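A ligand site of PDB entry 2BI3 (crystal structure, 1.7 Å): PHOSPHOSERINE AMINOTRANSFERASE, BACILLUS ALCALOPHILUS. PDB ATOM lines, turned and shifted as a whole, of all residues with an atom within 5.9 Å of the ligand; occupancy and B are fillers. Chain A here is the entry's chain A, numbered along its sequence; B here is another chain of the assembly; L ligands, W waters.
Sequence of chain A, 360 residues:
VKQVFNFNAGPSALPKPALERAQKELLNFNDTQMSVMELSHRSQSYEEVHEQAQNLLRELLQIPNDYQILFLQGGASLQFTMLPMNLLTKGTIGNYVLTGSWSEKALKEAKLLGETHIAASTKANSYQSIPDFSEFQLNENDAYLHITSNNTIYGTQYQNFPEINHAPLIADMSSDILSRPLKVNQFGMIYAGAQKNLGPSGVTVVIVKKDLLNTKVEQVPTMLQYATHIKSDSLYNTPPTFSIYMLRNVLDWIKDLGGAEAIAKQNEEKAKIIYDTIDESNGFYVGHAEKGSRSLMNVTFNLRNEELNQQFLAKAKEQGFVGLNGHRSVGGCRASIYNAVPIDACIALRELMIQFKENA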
ATOM      1  N   ALA A   9      16.175  23.946   4.403  1.00  0.00           N
ATOM      2  CA  ALA A   9      15.993  23.623   5.811  1.00  0.00           C
ATOM      3  C   ALA A   9      15.249  22.337   6.079  1.00  0.00           C
ATOM      4  O   ALA A   9      15.140  21.905   7.241  1.00  0.00           O
ATOM      5  CB  ALA A   9      15.286  24.799   6.521  1.00  0.00           C
ATOM      6  N   GLY A  74       4.580   9.764   9.520  1.00  0.00           N
ATOM      7  CA  GLY A  74       3.796  10.800  10.159  1.00  0.00           C
ATOM      8  C   GLY A  74       4.599  12.032  10.530  1.00  0.00           C
ATOM      9  O   GLY A  74       4.013  13.062  10.906  1.00  0.00           O
ATOM     10  N   GLY A  75       5.920  11.933  10.443  1.00  0.00           N
ATOM     11  CA  GLY A  75       6.740  13.107  10.748  1.00  0.00           C
ATOM     12  C   GLY A  75       6.871  13.342  12.246  1.00  0.00           C
ATOM     13  O   GLY A  75       6.247  12.713  13.099  1.00  0.00           O
ATOM     14  N   ALA A  76       7.742  14.312  12.567  1.00  0.00           N
ATOM     15  CA  ALA A  76       7.894  14.663  13.984  1.00  0.00           C
ATOM     16  C   ALA A  76       6.559  15.152  14.512  1.00  0.00           C
ATOM     17  O   ALA A  76       6.180  14.983  15.672  1.00  0.00           O
ATOM     18  CB  ALA A  76       8.987  15.714  14.128  1.00  0.00           C
ATOM     19  N   SER A  77       5.824  15.796  13.614  1.00  0.00           N
ATOM     20  CA  SER A  77       4.534  16.357  14.033  1.00  0.00           C
ATOM     21  C   SER A  77       3.607  15.313  14.593  1.00  0.00           C
ATOM     22  O   SER A  77       2.920  15.577  15.584  1.00  0.00           O
ATOM     23  CB  SER A  77       3.854  17.108  12.880  1.00  0.00           C
ATOM     24  OG  SER A  77       4.635  18.247  12.572  1.00  0.00           O
ATOM     25  N   LEU A  78       3.584  14.100  14.014  1.00  0.00           N
ATOM     26  CA  LEU A  78       2.740  13.072  14.601  1.00  0.00           C
ATOM     27  C   LEU A  78       3.267  12.660  15.987  1.00  0.00           C
ATOM     28  O   LEU A  78       2.503  12.277  16.874  1.00  0.00           O
ATOM     29  CB  LEU A  78       2.633  11.830  13.711  1.00  0.00           C
ATOM     30  CG  LEU A  78       1.676  10.754  14.240  1.00  0.00           C
ATOM     31  CD1 LEU A  78       0.295  11.343  14.497  1.00  0.00           C
ATOM     32  CD2 LEU A  78       1.588   9.575  13.280  1.00  0.00           C
ATOM     33  N   PHE A  80       4.469  14.605  18.169  1.00  0.00           N
ATOM     34  CA  PHE A  80       3.957  15.573  19.136  1.00  0.00           C
ATOM     35  C   PHE A  80       2.682  15.094  19.832  1.00  0.00           C
ATOM     36  O   PHE A  80       2.464  15.361  21.011  1.00  0.00           O
ATOM     37  CB  PHE A  80       3.664  16.918  18.468  1.00  0.00           C
ATOM     38  CG  PHE A  80       4.828  17.704  17.902  1.00  0.00           C
ATOM     39  CD1 PHE A  80       4.586  18.721  16.987  1.00  0.00           C
ATOM     40  CD2 PHE A  80       6.139  17.397  18.269  1.00  0.00           C
ATOM     41  CE1 PHE A  80       5.631  19.464  16.436  1.00  0.00           C
ATOM     42  CE2 PHE A  80       7.171  18.149  17.752  1.00  0.00           C
ATOM     43  CZ  PHE A  80       6.919  19.170  16.850  1.00  0.00           C
ATOM     44  N   TRP A 102       9.052  25.064  17.359  1.00  0.00           N
ATOM     45  CA  TRP A 102       8.766  23.625  17.416  1.00  0.00           C
ATOM     46  C   TRP A 102       8.491  23.177  18.845  1.00  0.00           C
ATOM     47  O   TRP A 102       7.651  22.299  19.067  1.00  0.00           O
ATOM     48  CB  TRP A 102       9.885  22.782  16.800  1.00  0.00           C
ATOM     49  CG  TRP A 102       9.949  23.029  15.317  1.00  0.00           C
ATOM     50  CD1 TRP A 102      10.964  23.611  14.609  1.00  0.00           C
ATOM     51  CD2 TRP A 102       8.939  22.695  14.377  1.00  0.00           C
ATOM     52  NE1 TRP A 102      10.645  23.651  13.274  1.00  0.00           N
ATOM     53  CE2 TRP A 102       9.401  23.093  13.108  1.00  0.00           C
ATOM     54  CE3 TRP A 102       7.686  22.082  14.480  1.00  0.00           C
ATOM     55  CZ2 TRP A 102       8.653  22.900  11.938  1.00  0.00           C
ATOM     56  CZ3 TRP A 102       6.957  21.900  13.322  1.00  0.00           C
ATOM     57  CH2 TRP A 102       7.422  22.303  12.061  1.00  0.00           C
ATOM     58  N   THR A 148      13.488  20.424  22.938  1.00  0.00           N
ATOM     59  CA  THR A 148      13.807  20.502  21.511  1.00  0.00           C
ATOM     60  C   THR A 148      15.312  20.742  21.411  1.00  0.00           C
ATOM     61  O   THR A 148      15.775  21.848  21.707  1.00  0.00           O
ATOM     62  CB  THR A 148      12.995  21.591  20.842  1.00  0.00           C
ATOM     63  OG1 THR A 148      11.625  21.416  21.252  1.00  0.00           O
ATOM     64  CG2 THR A 148      13.035  21.500  19.313  1.00  0.00           C
ATOM     65  N   ASN A 150      17.558  21.060  19.025  1.00  0.00           N
ATOM     66  CA  ASN A 150      17.935  22.099  18.071  1.00  0.00           C
ATOM     67  C   ASN A 150      16.687  22.828  17.577  1.00  0.00           C
ATOM     68  O   ASN A 150      15.751  22.233  17.024  1.00  0.00           O
ATOM     69  CB  ASN A 150      18.710  21.498  16.877  1.00  0.00           C
ATOM     70  CG  ASN A 150      19.252  22.582  15.954  1.00  0.00           C
ATOM     71  OD1 ASN A 150      18.678  22.899  14.898  1.00  0.00           O
ATOM     72  ND2 ASN A 150      20.366  23.206  16.301  1.00  0.00           N
ATOM     73  N   ASN A 151      16.658  24.148  17.798  1.00  0.00           N
ATOM     74  CA  ASN A 151      15.490  24.966  17.517  1.00  0.00           C
ATOM     75  C   ASN A 151      15.614  25.538  16.116  1.00  0.00           C
ATOM     76  O   ASN A 151      16.174  26.602  15.921  1.00  0.00           O
ATOM     77  CB  ASN A 151      15.364  26.051  18.612  1.00  0.00           C
ATOM     78  CG  ASN A 151      15.357  25.374  19.972  1.00  0.00           C
ATOM     79  OD1 ASN A 151      14.337  24.830  20.414  1.00  0.00           O
ATOM     80  ND2 ASN A 151      16.492  25.376  20.659  1.00  0.00           N
ATOM     81  N   THR A 152      15.065  24.757  15.175  1.00  0.00           N
ATOM     82  CA  THR A 152      15.341  24.898  13.758  1.00  0.00           C
ATOM     83  C   THR A 152      15.065  26.300  13.243  1.00  0.00           C
ATOM     84  O   THR A 152      15.739  26.816  12.348  1.00  0.00           O
ATOM     85  CB  THR A 152      14.470  23.880  12.990  1.00  0.00           C
ATOM     86  OG1 THR A 152      14.405  22.707  13.791  1.00  0.00           O
ATOM     87  CG2 THR A 152      15.115  23.485  11.668  1.00  0.00           C
ATOM     88  N   ASP A 172      12.888  16.154  20.979  1.00  0.00           N
ATOM     89  CA  ASP A 172      12.725  16.354  19.545  1.00  0.00           C
ATOM     90  C   ASP A 172      14.089  16.743  18.976  1.00  0.00           C
ATOM     91  O   ASP A 172      14.499  17.909  19.091  1.00  0.00           O
ATOM     92  CB  ASP A 172      11.683  17.416  19.266  1.00  0.00           C
ATOM     93  CG  ASP A 172      11.500  17.756  17.810  1.00  0.00           C
ATOM     94  OD1 ASP A 172      12.188  17.128  16.966  1.00  0.00           O
ATOM     95  OD2 ASP A 172      10.649  18.640  17.552  1.00  0.00           O
ATOM     96  N   MET A 173      14.749  15.762  18.352  1.00  0.00           N
ATOM     97  CA  MET A 173      16.063  16.060  17.759  1.00  0.00           C
ATOM     98  C   MET A 173      16.018  16.112  16.237  1.00  0.00           C
ATOM     99  O   MET A 173      17.063  15.863  15.644  1.00  0.00           O
ATOM    100  CB  MET A 173      17.065  14.992  18.187  1.00  0.00           C
ATOM    101  CG  MET A 173      17.320  15.007  19.701  1.00  0.00           C
ATOM    102  SD  MET A 173      18.744  13.968  20.107  1.00  0.00           S
ATOM    103  CE  MET A 173      18.839  14.233  21.889  1.00  0.00           C
ATOM    104  N   SER A 174      14.868  16.438  15.652  1.00  0.00           N
ATOM    105  CA  SER A 174      14.696  16.466  14.196  1.00  0.00           C
ATOM    106  C   SER A 174      15.854  17.142  13.483  1.00  0.00           C
ATOM    107  O   SER A 174      16.376  16.598  12.500  1.00  0.00           O
ATOM    108  CB  SER A 174      13.392  17.162  13.825  1.00  0.00           C
ATOM    109  OG  SER A 174      12.266  16.428  14.309  1.00  0.00           O
ATOM    110  N   SER A 175      16.294  18.326  13.968  1.00  0.00           N
ATOM    111  CA  SER A 175      17.286  19.021  13.133  1.00  0.00           C
ATOM    112  C   SER A 175      18.715  18.904  13.613  1.00  0.00           C
ATOM    113  O   SER A 175      19.561  19.585  13.014  1.00  0.00           O
ATOM    114  CB  SER A 175      16.898  20.496  12.948  1.00  0.00           C
ATOM    115  OG  SER A 175      16.565  21.086  14.200  1.00  0.00           O
ATOM    116  N   TYR A 191      13.221  11.541  19.178  1.00  0.00           N
ATOM    117  CA  TYR A 191      12.588  11.355  17.860  1.00  0.00           C
ATOM    118  C   TYR A 191      13.058  12.436  16.900  1.00  0.00           C
ATOM    119  O   TYR A 191      13.477  13.504  17.306  1.00  0.00           O
ATOM    120  CB  TYR A 191      11.075  11.321  18.003  1.00  0.00           C
ATOM    121  CG  TYR A 191      10.418  12.572  18.504  1.00  0.00           C
ATOM    122  CD1 TYR A 191       9.975  13.559  17.631  1.00  0.00           C
ATOM    123  CD2 TYR A 191      10.220  12.785  19.857  1.00  0.00           C
ATOM    124  CE1 TYR A 191       9.365  14.711  18.084  1.00  0.00           C
ATOM    125  CE2 TYR A 191       9.599  13.941  20.322  1.00  0.00           C
ATOM    126  CZ  TYR A 191       9.170  14.894  19.442  1.00  0.00           C
ATOM    127  OH  TYR A 191       8.566  16.048  19.867  1.00  0.00           O
ATOM    128  N   GLY A 193      12.135  13.639  12.589  1.00  0.00           N
ATOM    129  CA  GLY A 193      11.811  13.361  11.177  1.00  0.00           C
ATOM    130  C   GLY A 193      13.135  13.164  10.467  1.00  0.00           C
ATOM    131  O   GLY A 193      14.144  13.829  10.721  1.00  0.00           O
ATOM    132  N   GLN A 195      14.119  13.933   7.438  1.00  0.00           N
ATOM    133  CA  GLN A 195      14.386  14.816   6.310  1.00  0.00           C
ATOM    134  C   GLN A 195      15.299  15.971   6.648  1.00  0.00           C
ATOM    135  O   GLN A 195      15.639  16.788   5.784  1.00  0.00           O
ATOM    136  CB  GLN A 195      13.088  15.388   5.735  1.00  0.00           C
ATOM    137  CG  GLN A 195      12.364  16.355   6.693  1.00  0.00           C
ATOM    138  CD  GLN A 195      11.379  15.632   7.592  1.00  0.00           C
ATOM    139  OE1 GLN A 195      11.418  14.427   7.832  1.00  0.00           O
ATOM    140  NE2 GLN A 195      10.447  16.394   8.155  1.00  0.00           N
ATOM    141  N   LYS A 196      15.746  16.094   7.915  1.00  0.00           N
ATOM    142  CA  LYS A 196      16.692  17.226   8.026  1.00  0.00           C
ATOM    143  C   LYS A 196      18.119  16.757   8.020  1.00  0.00           C
ATOM    144  O   LYS A 196      18.990  17.278   7.320  1.00  0.00           O
ATOM    145  CB  LYS A 196      16.365  18.065   9.276  1.00  0.00           C
ATOM    146  CG  LYS A 196      14.877  18.265   9.458  1.00  0.00           C
ATOM    147  CD  LYS A 196      14.570  19.693   9.889  1.00  0.00           C
ATOM    148  CE  LYS A 196      13.225  20.119   9.336  1.00  0.00           C
ATOM    149  NZ  LYS A 196      12.288  20.475  10.439  1.00  0.00           N
ATOM    150  N   THR A 204      10.207   8.733  10.170  1.00  0.00           N
ATOM    151  CA  THR A 204      10.541   9.389  11.425  1.00  0.00           C
ATOM    152  C   THR A 204      11.286   8.392  12.312  1.00  0.00           C
ATOM    153  O   THR A 204      10.728   7.320  12.536  1.00  0.00           O
ATOM    154  CB  THR A 204       9.259   9.883  12.117  1.00  0.00           C
ATOM    155  OG1 THR A 204       8.715  10.938  11.329  1.00  0.00           O
ATOM    156  CG2 THR A 204       9.590  10.454  13.488  1.00  0.00           C
ATOM    157  N   TYR A 338      23.171  21.290   7.766  1.00  0.00           N
ATOM    158  CA  TYR A 338      23.124  19.915   8.249  1.00  0.00           C
ATOM    159  C   TYR A 338      24.329  19.090   7.791  1.00  0.00           C
ATOM    160  O   TYR A 338      25.091  19.585   6.956  1.00  0.00           O
ATOM    161  CB  TYR A 338      21.837  19.256   7.732  1.00  0.00           C
ATOM    162  CG  TYR A 338      20.586  19.986   8.130  1.00  0.00           C
ATOM    163  CD1 TYR A 338      19.732  20.523   7.176  1.00  0.00           C
ATOM    164  CD2 TYR A 338      20.234  20.136   9.459  1.00  0.00           C
ATOM    165  CE1 TYR A 338      18.579  21.190   7.525  1.00  0.00           C
ATOM    166  CE2 TYR A 338      19.080  20.806   9.829  1.00  0.00           C
ATOM    167  CZ  TYR A 338      18.246  21.333   8.865  1.00  0.00           C
ATOM    168  OH  TYR A 338      17.098  22.005   9.207  1.00  0.00           O
ATOM    169  N   HIS B  41       9.748  21.291   0.933  1.00  0.00           N
ATOM    170  CA  HIS B  41       8.364  21.086   0.511  1.00  0.00           C
ATOM    171  C   HIS B  41       7.645  22.416   0.345  1.00  0.00           C
ATOM    172  O   HIS B  41       6.504  22.494  -0.097  1.00  0.00           O
ATOM    173  CB  HIS B  41       7.661  20.195   1.530  1.00  0.00           C
ATOM    174  CG  HIS B  41       7.598  20.773   2.904  1.00  0.00           C
ATOM    175  ND1 HIS B  41       8.698  21.075   3.679  1.00  0.00           N
ATOM    176  CD2 HIS B  41       6.514  21.121   3.641  1.00  0.00           C
ATOM    177  CE1 HIS B  41       8.307  21.579   4.832  1.00  0.00           C
ATOM    178  NE2 HIS B  41       6.977  21.614   4.839  1.00  0.00           N
ATOM    179  N   GLN B  73       0.430  10.505   5.451  1.00  0.00           N
ATOM    180  CA  GLN B  73       1.271   9.400   5.864  1.00  0.00           C
ATOM    181  C   GLN B  73       0.489   8.442   6.766  1.00  0.00           C
ATOM    182  O   GLN B  73      -0.605   8.817   7.221  1.00  0.00           O
ATOM    183  CB  GLN B  73       2.498   9.942   6.620  1.00  0.00           C
ATOM    184  CG  GLN B  73       3.384  10.847   5.757  1.00  0.00           C
ATOM    185  CD  GLN B  73       4.605  11.291   6.577  1.00  0.00           C
ATOM    186  OE1 GLN B  73       5.440  10.440   6.929  1.00  0.00           O
ATOM    187  NE2 GLN B  73       4.668  12.584   6.874  1.00  0.00           N
ATOM    188  N   ASN B 237       2.432  19.617   7.534  1.00  0.00           N
ATOM    189  CA  ASN B 237       3.809  19.269   7.919  1.00  0.00           C
ATOM    190  C   ASN B 237       4.499  18.729   6.676  1.00  0.00           C
ATOM    191  O   ASN B 237       3.948  18.841   5.572  1.00  0.00           O
ATOM    192  CB  ASN B 237       3.898  18.301   9.081  1.00  0.00           C
ATOM    193  CG  ASN B 237       3.496  16.883   8.781  1.00  0.00           C
ATOM    194  OD1 ASN B 237       2.589  16.651   7.966  1.00  0.00           O
ATOM    195  ND2 ASN B 237       4.173  15.949   9.441  1.00  0.00           N
ATOM    196  N   THR B 238       5.683  18.199   6.831  1.00  0.00           N
ATOM    197  CA  THR B 238       6.459  17.793   5.660  1.00  0.00           C
ATOM    198  C   THR B 238       5.784  16.551   5.061  1.00  0.00           C
ATOM    199  O   THR B 238       5.635  15.547   5.755  1.00  0.00           O
ATOM    200  CB  THR B 238       7.913  17.481   6.035  1.00  0.00           C
ATOM    201  OG1 THR B 238       8.484  18.551   6.822  1.00  0.00           O
ATOM    202  CG2 THR B 238       8.800  17.354   4.801  1.00  0.00           C
HETATM  203  N1  LIG L   1      10.483  19.461  14.955  1.00  0.00           N
HETATM  204  C1  LIG L   1      11.604  20.093  14.513  1.00  0.00           C
HETATM  205  C2  LIG L   1      12.706  20.499  15.515  1.00  0.00           C
HETATM  206  C3  LIG L   1      11.748  20.364  13.187  1.00  0.00           C
HETATM  207  O1  LIG L   1      12.889  21.016  12.787  1.00  0.00           O
HETATM  208  C4  LIG L   1      10.736  20.025  12.312  1.00  0.00           C
HETATM  209  C5  LIG L   1      10.942  20.149  10.792  1.00  0.00           C
HETATM  210  C6  LIG L   1       9.618  19.364  12.759  1.00  0.00           C
HETATM  211  C7  LIG L   1       9.452  19.150  14.092  1.00  0.00           C
HETATM  212  C8  LIG L   1       8.483  18.972  11.795  1.00  0.00           C
HETATM  213  O2  LIG L   1       8.711  17.684  11.250  1.00  0.00           O
HETATM  214  P1  LIG L   1       7.609  17.057  10.267  1.00  0.00           P
HETATM  215  O3  LIG L   1       7.425  18.094   9.235  1.00  0.00           O
HETATM  216  O4  LIG L   1       6.428  16.871  11.152  1.00  0.00           O
HETATM  217  O5  LIG L   1       8.199  15.803   9.787  1.00  0.00           O
HETATM  218  O   HOH W   1      11.199  16.384  11.675  1.00  0.00           O
HETATM  219  O   HOH W   2       6.959  14.443   7.832  1.00  0.00           O
HETATM  220  O   HOH W   3       6.439  20.677   9.234  1.00  0.00           O
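A carbon (C5) of the ligand is covalently linked to the side-chain amino group (NZ) of Lys 196, 1.4 Å away.
An oxygen (O1) of the ligand is in hydrogen-bond range of the side-chain hydroxyl of Thr 152, at 2.5 Å.
The backbone NH (N) of Ser 77 lies within hydrogen-bond range of an oxygen (O4) of the ligand (2.8 Å).
The side-chain hydroxyl of Ser 77 sits at hydrogen-bond distance from an oxygen (O4) of the ligand (2.7 Å).
The backbone NH (N) of Thr 238 of chain B lies within hydrogen-bond range of an oxygen (O3) of the ligand, 3.0 Å away.
O3 of the ligand is in hydrogen-bond range of OG1 of Thr 238 of chain B (2.7 Å).
OD2 of Asp 172 lies within hydrogen-bond range of N1 of the ligand (2.7 Å).
The side-chain amide nitrogen (NE2) of Gln 195 lies within hydrogen-bond range of an oxygen (O5) of the ligand (2.8 Å).
ND2 of Asn 237 of chain B is in hydrogen-bond range of O4 of the ligand.
N of Ala 76 lies within hydrogen-bond range of O5 of the ligand, at 3.2 Å.
The indole nitrogen of Trp 102 lies close to an oxygen (O1) of the ligand (3.5 Å).
CA of Gly 75 touches O5 of the ligand, 3.2 Å away.
CZ of Phe 80 touches C7 of the ligand, 3.7 Å away.
Thr 148 touches the ligand.
O of Asn 150 touches C2 of the ligand, at 3.8 Å.
Ser 174 touches the ligand (CB to C1, 3.5 Å).
Ser 175 touches the ligand.
Within 4 Å of the ligand: Gly 75, Ala 76, Ser 77, Phe 80, Trp 102, Thr 148, Asn 150, Thr 152, Asp 172, Ser 174, Ser 175, Gln 195, Lys 196, Asn 237 of chain B and Thr 238 of chain B.
The nearest printed residue that does not touch the ligand is Gly 74 (4.5 Å).
The side-chain hydroxyl (OG1) of Thr 152 is in hydrogen-bond range of the side-chain hydroxyl (OG) of Ser 175.
The side-chain amide nitrogen (NE2) of Gln 195 is in hydrogen-bond range of the side-chain hydroxyl (OG1) of Thr 238 of chain B (3.2 Å).
NE2 of Gln 73 of chain B sits at hydrogen-bond distance from O of Thr 238 of chain B (3.3 Å).
OD1 of Asp 172 lies within hydrogen-bond range of OG of Ser 174 (2.7 Å).
The side-chain amide nitrogen of Asn 237 of chain B is in hydrogen-bond range of the backbone carbonyl oxygen of Gly 74, 3.2 Å away.
N of Gly 75 sits close to OG1 of Thr 204, at 3.1 Å.
OG of Ser 174 lies within hydrogen-bond range of N of Gly 193 (3.3 Å).
OD1 of Asn 150 lies within hydrogen-bond range of OG of Ser 175 (2.9 Å).
Water W2 lies within hydrogen-bond range of O5 of the ligand (2.7 Å), O of Thr 238 of chain B (2.7 Å) and NE2 of Gln 73 of chain B (3.1 Å).
Water W1 lies within hydrogen-bond range of O2 of the ligand, OG of Ser 174 and N of Gly 193.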
